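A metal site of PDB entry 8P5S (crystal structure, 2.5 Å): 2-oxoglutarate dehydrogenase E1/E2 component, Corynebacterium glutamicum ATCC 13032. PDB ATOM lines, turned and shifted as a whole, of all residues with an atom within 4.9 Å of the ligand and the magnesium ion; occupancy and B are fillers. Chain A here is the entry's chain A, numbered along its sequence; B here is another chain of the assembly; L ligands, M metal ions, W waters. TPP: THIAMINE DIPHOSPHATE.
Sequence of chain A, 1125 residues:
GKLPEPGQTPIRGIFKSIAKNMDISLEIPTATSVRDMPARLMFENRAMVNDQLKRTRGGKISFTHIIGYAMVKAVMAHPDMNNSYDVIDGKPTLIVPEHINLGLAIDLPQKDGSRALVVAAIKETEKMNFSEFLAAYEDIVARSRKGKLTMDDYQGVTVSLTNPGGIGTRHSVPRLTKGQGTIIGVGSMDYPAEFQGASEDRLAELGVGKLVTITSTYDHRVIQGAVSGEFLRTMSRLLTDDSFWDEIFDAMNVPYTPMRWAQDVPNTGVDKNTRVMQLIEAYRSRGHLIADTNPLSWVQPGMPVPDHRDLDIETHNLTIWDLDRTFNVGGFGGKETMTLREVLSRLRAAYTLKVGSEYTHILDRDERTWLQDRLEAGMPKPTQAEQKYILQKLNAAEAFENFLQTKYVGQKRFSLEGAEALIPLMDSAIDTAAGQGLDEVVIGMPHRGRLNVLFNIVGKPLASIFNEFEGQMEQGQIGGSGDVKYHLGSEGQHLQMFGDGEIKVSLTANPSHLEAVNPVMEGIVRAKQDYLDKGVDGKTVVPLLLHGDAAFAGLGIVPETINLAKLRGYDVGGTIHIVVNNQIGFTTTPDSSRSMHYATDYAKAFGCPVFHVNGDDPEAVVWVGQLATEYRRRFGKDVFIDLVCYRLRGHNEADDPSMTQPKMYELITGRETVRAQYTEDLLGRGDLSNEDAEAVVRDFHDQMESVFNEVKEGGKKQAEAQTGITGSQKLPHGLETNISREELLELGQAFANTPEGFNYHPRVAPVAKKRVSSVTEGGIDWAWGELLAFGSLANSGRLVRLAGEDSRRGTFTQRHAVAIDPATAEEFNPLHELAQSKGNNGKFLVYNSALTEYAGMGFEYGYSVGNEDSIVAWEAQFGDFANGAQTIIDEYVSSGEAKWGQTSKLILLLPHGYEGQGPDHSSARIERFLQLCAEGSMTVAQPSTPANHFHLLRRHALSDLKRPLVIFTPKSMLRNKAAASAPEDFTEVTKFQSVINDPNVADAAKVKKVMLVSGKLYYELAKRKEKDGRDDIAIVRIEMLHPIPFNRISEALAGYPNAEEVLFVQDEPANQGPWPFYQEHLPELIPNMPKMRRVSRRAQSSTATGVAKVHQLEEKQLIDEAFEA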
ATOM      1  N   HIS A 447      35.300   9.119 -25.690  1.00  0.00           N
ATOM      2  CA  HIS A 447      34.991  10.390 -26.335  1.00  0.00           C
ATOM      3  C   HIS A 447      34.294  11.419 -25.443  1.00  0.00           C
ATOM      4  O   HIS A 447      34.575  12.601 -25.593  1.00  0.00           O
ATOM      5  CB  HIS A 447      34.146  10.151 -27.601  1.00  0.00           C
ATOM      6  CG  HIS A 447      32.892   9.356 -27.374  1.00  0.00           C
ATOM      7  ND1 HIS A 447      32.934   7.995 -27.137  1.00  0.00           N
ATOM      8  CD2 HIS A 447      31.594   9.765 -27.378  1.00  0.00           C
ATOM      9  CE1 HIS A 447      31.672   7.621 -26.963  1.00  0.00           C
ATOM     10  NE2 HIS A 447      30.832   8.648 -27.099  1.00  0.00           N
ATOM     11  N   ARG A 448      33.359  11.026 -24.585  1.00  0.00           N
ATOM     12  CA  ARG A 448      32.582  11.983 -23.782  1.00  0.00           C
ATOM     13  C   ARG A 448      33.435  12.944 -22.956  1.00  0.00           C
ATOM     14  O   ARG A 448      34.109  12.530 -22.023  1.00  0.00           O
ATOM     15  CB  ARG A 448      31.615  11.242 -22.833  1.00  0.00           C
ATOM     16  CG  ARG A 448      30.665  12.165 -22.059  1.00  0.00           C
ATOM     17  CD  ARG A 448      29.446  11.477 -21.458  1.00  0.00           C
ATOM     18  NE  ARG A 448      28.750  10.572 -22.384  1.00  0.00           N
ATOM     19  CZ  ARG A 448      27.790  10.936 -23.221  1.00  0.00           C
ATOM     20  NH1 ARG A 448      27.228  10.052 -24.021  1.00  0.00           N
ATOM     21  NH2 ARG A 448      27.377  12.197 -23.270  1.00  0.00           N
ATOM     22  N   SER A 512      37.337   3.603 -31.278  1.00  0.00           N
ATOM     23  CA  SER A 512      35.974   3.774 -30.770  1.00  0.00           C
ATOM     24  C   SER A 512      35.513   2.562 -29.956  1.00  0.00           C
ATOM     25  O   SER A 512      34.591   2.705 -29.159  1.00  0.00           O
ATOM     26  CB  SER A 512      34.990   4.056 -31.889  1.00  0.00           C
ATOM     27  OG  SER A 512      35.374   5.234 -32.581  1.00  0.00           O
ATOM     28  N   HIS A 513      36.156   1.392 -30.108  1.00  0.00           N
ATOM     29  CA  HIS A 513      35.879   0.207 -29.283  1.00  0.00           C
ATOM     30  C   HIS A 513      36.156   0.570 -27.828  1.00  0.00           C
ATOM     31  O   HIS A 513      37.287   0.881 -27.477  1.00  0.00           O
ATOM     32  CB  HIS A 513      36.782  -0.973 -29.723  1.00  0.00           C
ATOM     33  CG  HIS A 513      36.517  -1.498 -31.098  1.00  0.00           C
ATOM     34  ND1 HIS A 513      36.518  -0.652 -32.205  1.00  0.00           N
ATOM     35  CD2 HIS A 513      36.292  -2.762 -31.513  1.00  0.00           C
ATOM     36  CE1 HIS A 513      36.280  -1.431 -33.254  1.00  0.00           C
ATOM     37  NE2 HIS A 513      36.118  -2.703 -32.880  1.00  0.00           N
ATOM     38  N   LEU A 514      35.094   0.689 -27.044  1.00  0.00           N
ATOM     39  CA  LEU A 514      35.214   1.113 -25.665  1.00  0.00           C
ATOM     40  C   LEU A 514      36.064   0.157 -24.840  1.00  0.00           C
ATOM     41  O   LEU A 514      36.104  -1.054 -25.109  1.00  0.00           O
ATOM     42  CB  LEU A 514      33.815   1.243 -25.057  1.00  0.00           C
ATOM     43  CG  LEU A 514      32.915   2.336 -25.660  1.00  0.00           C
ATOM     44  CD1 LEU A 514      31.472   2.232 -25.149  1.00  0.00           C
ATOM     45  CD2 LEU A 514      33.499   3.736 -25.418  1.00  0.00           C
ATOM     46  N   GLY A 548      32.804   4.615 -18.839  1.00  0.00           N
ATOM     47  CA  GLY A 548      31.364   4.828 -18.809  1.00  0.00           C
ATOM     48  C   GLY A 548      30.762   3.672 -17.996  1.00  0.00           C
ATOM     49  O   GLY A 548      31.347   2.593 -17.943  1.00  0.00           O
ATOM     50  N   ASP A 549      29.617   3.871 -17.348  1.00  0.00           N
ATOM     51  CA  ASP A 549      29.011   2.849 -16.488  1.00  0.00           C
ATOM     52  C   ASP A 549      28.577   1.587 -17.228  1.00  0.00           C
ATOM     53  O   ASP A 549      28.665   0.510 -16.643  1.00  0.00           O
ATOM     54  CB  ASP A 549      27.818   3.414 -15.723  1.00  0.00           C
ATOM     55  CG  ASP A 549      26.800   4.096 -16.623  1.00  0.00           C
ATOM     56  OD1 ASP A 549      27.122   5.174 -17.163  1.00  0.00           O
ATOM     57  OD2 ASP A 549      25.679   3.553 -16.764  1.00  0.00           O
ATOM     58  N   ALA A 550      28.067   1.715 -18.438  1.00  0.00           N
ATOM     59  CA  ALA A 550      27.605   0.544 -19.182  1.00  0.00           C
ATOM     60  C   ALA A 550      28.798  -0.290 -19.665  1.00  0.00           C
ATOM     61  O   ALA A 550      28.791  -1.522 -19.532  1.00  0.00           O
ATOM     62  CB  ALA A 550      26.749   0.997 -20.366  1.00  0.00           C
ATOM     63  N   ALA A 551      29.842   0.385 -20.164  1.00  0.00           N
ATOM     64  CA  ALA A 551      31.041  -0.266 -20.674  1.00  0.00           C
ATOM     65  C   ALA A 551      31.909  -0.871 -19.575  1.00  0.00           C
ATOM     66  O   ALA A 551      32.504  -1.929 -19.788  1.00  0.00           O
ATOM     67  CB  ALA A 551      31.861   0.725 -21.472  1.00  0.00           C
ATOM     68  N   LEU A 555      32.026  -4.998 -20.476  1.00  0.00           N
ATOM     69  CA  LEU A 555      33.141  -5.520 -21.260  1.00  0.00           C
ATOM     70  C   LEU A 555      34.144  -6.203 -20.363  1.00  0.00           C
ATOM     71  O   LEU A 555      34.558  -5.613 -19.375  1.00  0.00           O
ATOM     72  CB  LEU A 555      33.788  -4.390 -22.072  1.00  0.00           C
ATOM     73  CG  LEU A 555      32.906  -3.853 -23.188  1.00  0.00           C
ATOM     74  CD1 LEU A 555      33.412  -2.527 -23.699  1.00  0.00           C
ATOM     75  CD2 LEU A 555      32.765  -4.856 -24.319  1.00  0.00           C
ATOM     76  N   VAL A 580      32.179   7.566 -14.991  1.00  0.00           N
ATOM     77  CA  VAL A 580      31.167   8.574 -15.208  1.00  0.00           C
ATOM     78  C   VAL A 580      29.843   7.821 -15.335  1.00  0.00           C
ATOM     79  O   VAL A 580      29.463   7.366 -16.411  1.00  0.00           O
ATOM     80  CB  VAL A 580      31.500   9.431 -16.449  1.00  0.00           C
ATOM     81  CG1 VAL A 580      30.445  10.491 -16.689  1.00  0.00           C
ATOM     82  CG2 VAL A 580      32.872  10.061 -16.300  1.00  0.00           C
ATOM     83  N   ASN A 582      26.412   7.854 -15.571  1.00  0.00           N
ATOM     84  CA  ASN A 582      25.252   8.679 -15.889  1.00  0.00           C
ATOM     85  C   ASN A 582      23.947   7.867 -15.975  1.00  0.00           C
ATOM     86  O   ASN A 582      22.971   8.348 -16.531  1.00  0.00           O
ATOM     87  CB  ASN A 582      25.480   9.483 -17.164  1.00  0.00           C
ATOM     88  CG  ASN A 582      25.904   8.683 -18.364  1.00  0.00           C
ATOM     89  OD1 ASN A 582      25.756   7.463 -18.422  1.00  0.00           O
ATOM     90  ND2 ASN A 582      26.449   9.367 -19.344  1.00  0.00           N
ATOM     91  N   GLN A 583      23.951   6.639 -15.422  1.00  0.00           N
ATOM     92  CA  GLN A 583      22.832   5.732 -15.250  1.00  0.00           C
ATOM     93  C   GLN A 583      22.107   5.416 -16.557  1.00  0.00           C
ATOM     94  O   GLN A 583      20.908   5.143 -16.536  1.00  0.00           O
ATOM     95  CB  GLN A 583      21.861   6.326 -14.212  1.00  0.00           C
ATOM     96  CG  GLN A 583      22.581   6.834 -12.965  1.00  0.00           C
ATOM     97  CD  GLN A 583      21.648   7.480 -11.997  1.00  0.00           C
ATOM     98  OE1 GLN A 583      20.698   6.858 -11.526  1.00  0.00           O
ATOM     99  NE2 GLN A 583      21.897   8.728 -11.668  1.00  0.00           N
ATOM    100  N   ILE A 584      22.829   5.426 -17.672  1.00  0.00           N
ATOM    101  CA  ILE A 584      22.324   5.107 -19.000  1.00  0.00           C
ATOM    102  C   ILE A 584      23.505   4.749 -19.942  1.00  0.00           C
ATOM    103  O   ILE A 584      24.657   5.140 -19.708  1.00  0.00           O
ATOM    104  CB  ILE A 584      21.472   6.287 -19.542  1.00  0.00           C
ATOM    105  CG1 ILE A 584      20.599   5.855 -20.732  1.00  0.00           C
ATOM    106  CG2 ILE A 584      22.320   7.491 -19.854  1.00  0.00           C
ATOM    107  CD1 ILE A 584      19.532   6.771 -21.041  1.00  0.00           C
ATOM    108  N   GLY A 585      23.206   3.968 -20.971  1.00  0.00           N
ATOM    109  CA  GLY A 585      24.141   3.564 -22.015  1.00  0.00           C
ATOM    110  C   GLY A 585      23.376   3.509 -23.325  1.00  0.00           C
ATOM    111  O   GLY A 585      22.758   2.486 -23.622  1.00  0.00           O
ATOM    112  N   PHE A 586      23.391   4.614 -24.098  1.00  0.00           N
ATOM    113  CA  PHE A 586      22.659   4.832 -25.348  1.00  0.00           C
ATOM    114  C   PHE A 586      21.131   4.797 -25.002  1.00  0.00           C
ATOM    115  O   PHE A 586      20.635   5.793 -24.500  1.00  0.00           O
ATOM    116  CB  PHE A 586      23.100   3.868 -26.488  1.00  0.00           C
ATOM    117  CG  PHE A 586      22.736   4.304 -27.886  1.00  0.00           C
ATOM    118  CD1 PHE A 586      21.706   5.210 -28.116  1.00  0.00           C
ATOM    119  CD2 PHE A 586      23.409   3.799 -28.989  1.00  0.00           C
ATOM    120  CE1 PHE A 586      21.396   5.633 -29.401  1.00  0.00           C
ATOM    121  CE2 PHE A 586      23.067   4.198 -30.287  1.00  0.00           C
ATOM    122  CZ  PHE A 586      22.066   5.116 -30.482  1.00  0.00           C
ATOM    123  N   HIS A 651      21.893  10.359 -26.772  1.00  0.00           N
ATOM    124  CA  HIS A 651      23.171   9.750 -27.139  1.00  0.00           C
ATOM    125  C   HIS A 651      23.747  10.360 -28.423  1.00  0.00           C
ATOM    126  O   HIS A 651      24.970  10.459 -28.545  1.00  0.00           O
ATOM    127  CB  HIS A 651      23.046   8.238 -27.276  1.00  0.00           C
ATOM    128  CG  HIS A 651      24.344   7.524 -27.506  1.00  0.00           C
ATOM    129  ND1 HIS A 651      25.231   7.278 -26.470  1.00  0.00           N
ATOM    130  CD2 HIS A 651      24.871   7.029 -28.646  1.00  0.00           C
ATOM    131  CE1 HIS A 651      26.255   6.634 -27.013  1.00  0.00           C
ATOM    132  NE2 HIS A 651      26.082   6.464 -28.326  1.00  0.00           N
ATOM    133  N   GLU B 805      22.878  -4.684 -28.680  1.00  0.00           N
ATOM    134  CA  GLU B 805      22.914  -3.390 -28.018  1.00  0.00           C
ATOM    135  C   GLU B 805      21.886  -2.439 -28.609  1.00  0.00           C
ATOM    136  O   GLU B 805      21.946  -2.142 -29.813  1.00  0.00           O
ATOM    137  CB  GLU B 805      24.314  -2.784 -28.097  1.00  0.00           C
ATOM    138  CG  GLU B 805      25.315  -3.529 -27.244  1.00  0.00           C
ATOM    139  CD  GLU B 805      26.768  -3.347 -27.639  1.00  0.00           C
ATOM    140  OE1 GLU B 805      27.056  -2.500 -28.499  1.00  0.00           O
ATOM    141  OE2 GLU B 805      27.619  -4.077 -27.082  1.00  0.00           O
ATOM    142  N   ASP B 806      20.927  -1.988 -27.779  1.00  0.00           N
ATOM    143  CA  ASP B 806      19.874  -1.017 -28.112  1.00  0.00           C
ATOM    144  C   ASP B 806      18.999  -1.529 -29.253  1.00  0.00           C
ATOM    145  O   ASP B 806      18.596  -0.772 -30.119  1.00  0.00           O
ATOM    146  CB  ASP B 806      20.513   0.332 -28.488  1.00  0.00           C
ATOM    147  CG  ASP B 806      21.487   0.805 -27.436  1.00  0.00           C
ATOM    148  OD1 ASP B 806      21.019   1.294 -26.386  1.00  0.00           O
ATOM    149  OD2 ASP B 806      22.724   0.659 -27.654  1.00  0.00           O
ATOM    150  N   LEU B 851      26.602  -4.293 -22.608  1.00  0.00           N
ATOM    151  CA  LEU B 851      27.656  -3.817 -23.484  1.00  0.00           C
ATOM    152  C   LEU B 851      28.706  -4.920 -23.568  1.00  0.00           C
ATOM    153  O   LEU B 851      29.671  -4.941 -22.785  1.00  0.00           O
ATOM    154  CB  LEU B 851      28.225  -2.532 -22.865  1.00  0.00           C
ATOM    155  CG  LEU B 851      29.007  -1.504 -23.704  1.00  0.00           C
ATOM    156  CD1 LEU B 851      29.341  -1.950 -25.120  1.00  0.00           C
ATOM    157  CD2 LEU B 851      28.391  -0.144 -23.586  1.00  0.00           C
ATOM    158  N   GLU B 853      30.322  -8.058 -26.663  1.00  0.00           N
ATOM    159  CA  GLU B 853      30.292  -8.684 -27.975  1.00  0.00           C
ATOM    160  C   GLU B 853      30.652 -10.154 -27.862  1.00  0.00           C
ATOM    161  O   GLU B 853      29.983 -10.984 -28.443  1.00  0.00           O
ATOM    162  CB  GLU B 853      31.227  -7.992 -28.965  1.00  0.00           C
ATOM    163  CG  GLU B 853      30.608  -6.746 -29.552  1.00  0.00           C
ATOM    164  CD  GLU B 853      30.875  -5.518 -28.707  1.00  0.00           C
ATOM    165  OE1 GLU B 853      31.946  -5.463 -28.066  1.00  0.00           O
ATOM    166  OE2 GLU B 853      30.019  -4.604 -28.702  1.00  0.00           O
ATOM    167  N   GLN B 877      26.117  -3.204 -32.668  1.00  0.00           N
ATOM    168  CA  GLN B 877      25.834  -1.762 -32.753  1.00  0.00           C
ATOM    169  C   GLN B 877      26.296  -1.247 -34.130  1.00  0.00           C
ATOM    170  O   GLN B 877      25.523  -0.692 -34.890  1.00  0.00           O
ATOM    171  CB  GLN B 877      26.463  -0.997 -31.590  1.00  0.00           C
ATOM    172  CG  GLN B 877      26.129   0.471 -31.606  1.00  0.00           C
ATOM    173  CD  GLN B 877      25.381   0.887 -30.365  1.00  0.00           C
ATOM    174  OE1 GLN B 877      25.846   1.725 -29.608  1.00  0.00           O
ATOM    175  NE2 GLN B 877      24.216   0.295 -30.152  1.00  0.00           N
ATOM    176  N   PHE B 881      32.562  -3.574 -34.386  1.00  0.00           N
ATOM    177  CA  PHE B 881      32.787  -4.021 -33.013  1.00  0.00           C
ATOM    178  C   PHE B 881      32.710  -5.540 -32.853  1.00  0.00           C
ATOM    179  O   PHE B 881      32.980  -6.023 -31.764  1.00  0.00           O
ATOM    180  CB  PHE B 881      31.788  -3.358 -32.048  1.00  0.00           C
ATOM    181  CG  PHE B 881      31.936  -1.869 -32.068  1.00  0.00           C
ATOM    182  CD1 PHE B 881      33.179  -1.287 -31.898  1.00  0.00           C
ATOM    183  CD2 PHE B 881      30.846  -1.044 -32.291  1.00  0.00           C
ATOM    184  CE1 PHE B 881      33.329   0.094 -31.928  1.00  0.00           C
ATOM    185  CE2 PHE B 881      30.998   0.335 -32.330  1.00  0.00           C
ATOM    186  CZ  PHE B 881      32.237   0.895 -32.169  1.00  0.00           C
HETATM  187  N1' TPP L   1      31.016  -1.986 -28.231  1.00  0.00           N
HETATM  188  C2' TPP L   1      32.231  -1.415 -28.146  1.00  0.00           C
HETATM  189  CM2 TPP L   1      33.371  -2.305 -27.765  1.00  0.00           C
HETATM  190  N3' TPP L   1      32.505  -0.128 -28.379  1.00  0.00           N
HETATM  191  C4' TPP L   1      31.491   0.678 -28.739  1.00  0.00           C
HETATM  192  N4' TPP L   1      31.803   1.947 -29.024  1.00  0.00           N
HETATM  193  C5' TPP L   1      30.159   0.183 -28.852  1.00  0.00           C
HETATM  194  C6' TPP L   1      30.013  -1.163 -28.580  1.00  0.00           C
HETATM  195  C7' TPP L   1      28.976   1.043 -29.218  1.00  0.00           C
HETATM  196  N3  TPP L   1      28.690   2.107 -28.224  1.00  0.00           N
HETATM  197  C2  TPP L   1      29.110   3.352 -28.333  1.00  0.00           C
HETATM  198  S1  TPP L   1      28.656   4.305 -27.031  1.00  0.00           S
HETATM  199  C5  TPP L   1      27.862   2.975 -26.277  1.00  0.00           C
HETATM  200  C4  TPP L   1      27.956   1.867 -27.057  1.00  0.00           C
HETATM  201  CM4 TPP L   1      27.301   0.539 -26.809  1.00  0.00           C
HETATM  202  C6  TPP L   1      27.237   3.105 -24.913  1.00  0.00           C
HETATM  203  C7  TPP L   1      28.209   3.605 -23.865  1.00  0.00           C
HETATM  204  O7  TPP L   1      27.577   3.494 -22.560  1.00  0.00           O
HETATM  205  PA  TPP L   1      28.376   3.970 -21.255  1.00  0.00           P
HETATM  206  O1A TPP L   1      29.583   3.117 -21.151  1.00  0.00           O
HETATM  207  O2A TPP L   1      27.469   4.091 -20.086  1.00  0.00           O
HETATM  208  O3A TPP L   1      28.838   5.425 -21.736  1.00  0.00           O
HETATM  209  PB  TPP L   1      28.118   6.878 -21.882  1.00  0.00           P
HETATM  210  O1B TPP L   1      29.152   7.830 -21.297  1.00  0.00           O
HETATM  211  O2B TPP L   1      27.853   7.128 -23.346  1.00  0.00           O
HETATM  212  O3B TPP L   1      26.856   6.784 -21.053  1.00  0.00           O
HETATM  213 MG    MG M   1      26.701   5.714 -19.257  1.00  0.00          MG
HETATM  214  O   HOH W   1      24.873   7.111 -23.750  1.00  0.00           O
HETATM  215  O   HOH W   2      30.571   3.703 -31.052  1.00  0.00           O
HETATM  216  O   HOH W   3      28.697   7.090 -18.681  1.00  0.00           O
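The side-chain amide nitrogen (NE2) of Gln 877 of chain B sits at hydrogen-bond distance from the side-chain carboxylate (OD2) of Asp 806 of chain B (2.9 Å). NE2 of Gln 877 of chain B is in hydrogen-bond range of O of Glu 805 of chain B, at 3.3 Å. O of Leu 851 of chain B lies within hydrogen-bond range of N of Leu 555, at 3.3 Å.
A nitrogen (N3) of the ligand sits close to the side-chain amide oxygen (OE1) of Gln 877 of chain B (3.2 Å). His 513 touches the ligand. CA of Gly 548 touches O1A of the ligand, 3.4 Å away. Gly 585 touches the ligand (CA to O7, 3.5 Å). Glu 805 of chain B touches the ligand. Leu 851 of chain B touches the ligand. Phe 881 of chain B touches the ligand. Hydrophobic or aromatic side chains within 4 Å of the ligand: Leu 514, Ala 550, Ala 551, His 651, Leu 851 of chain B and Phe 881 of chain B. 17 residues have an atom within 4 Å of the ligand: Arg 448, Ser 512, His 513, Leu 514, Gly 548, Asp 549, Ala 550, Ala 551, Asn 582, Ile 584, Gly 585, His 651, Glu 805 of chain B, Leu 851 of chain B, Glu 853 of chain B, Gln 877 of chain B and Phe 881 of chain B. The nearest printed residue that does not touch the ligand is Leu 555 (4.1 Å).
The backbone NH of Leu 514 sits at hydrogen-bond distance from a nitrogen (N3') of the ligand, at 3.0 Å. N of Ala 551 sits at hydrogen-bond distance from O1A of the ligand (2.9 Å). The backbone NH (N) of Ala 550 lies within hydrogen-bond range of an oxygen (O1A) of the ligand (3.4 Å). A nitrogen (N1') of the ligand sits at hydrogen-bond distance from the side-chain carboxylate (OE2) of Glu 853 of chain B, at 2.8 Å. The guanidinium group of Arg 448 is in salt-bridge range of an oxygen (O1B) of the ligand (3.0 Å). An oxygen (O2A) of the ligand sits close to the backbone NH (N) of Asp 549, at 3.5 Å. NE2 of His 651 sits close to S1 of the ligand. N4' of the ligand sits at hydrogen-bond distance from O of Ser 512 (2.9 Å).
The magnesium ion is bound by an oxygen (O2A) of the ligand (2.0 Å), an oxygen (O3B) of the ligand (2.1 Å), the side-chain amide oxygen (OD1) of Asn 582 (2.2 Å), the backbone carbonyl oxygen (O) of Ile 584 (2.2 Å), the side-chain carboxylate (OD1) of Asp 549 (2.2 Å) and water W3 (2.5 Å).
The nearest printed residue that does not touch the magnesium ion is Gly 585 (4.3 Å).
Water W3 lies within hydrogen-bond range of the backbone carbonyl oxygen (O) of Val 580 (2.4 Å), an oxygen (O1B) of the ligand (2.8 Å) and the side-chain amide nitrogen (ND2) of Asn 582 (3.3 Å). Water W1 lies within hydrogen-bond range of ND1 of His 651, N of Phe 586 and O2B of the ligand.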
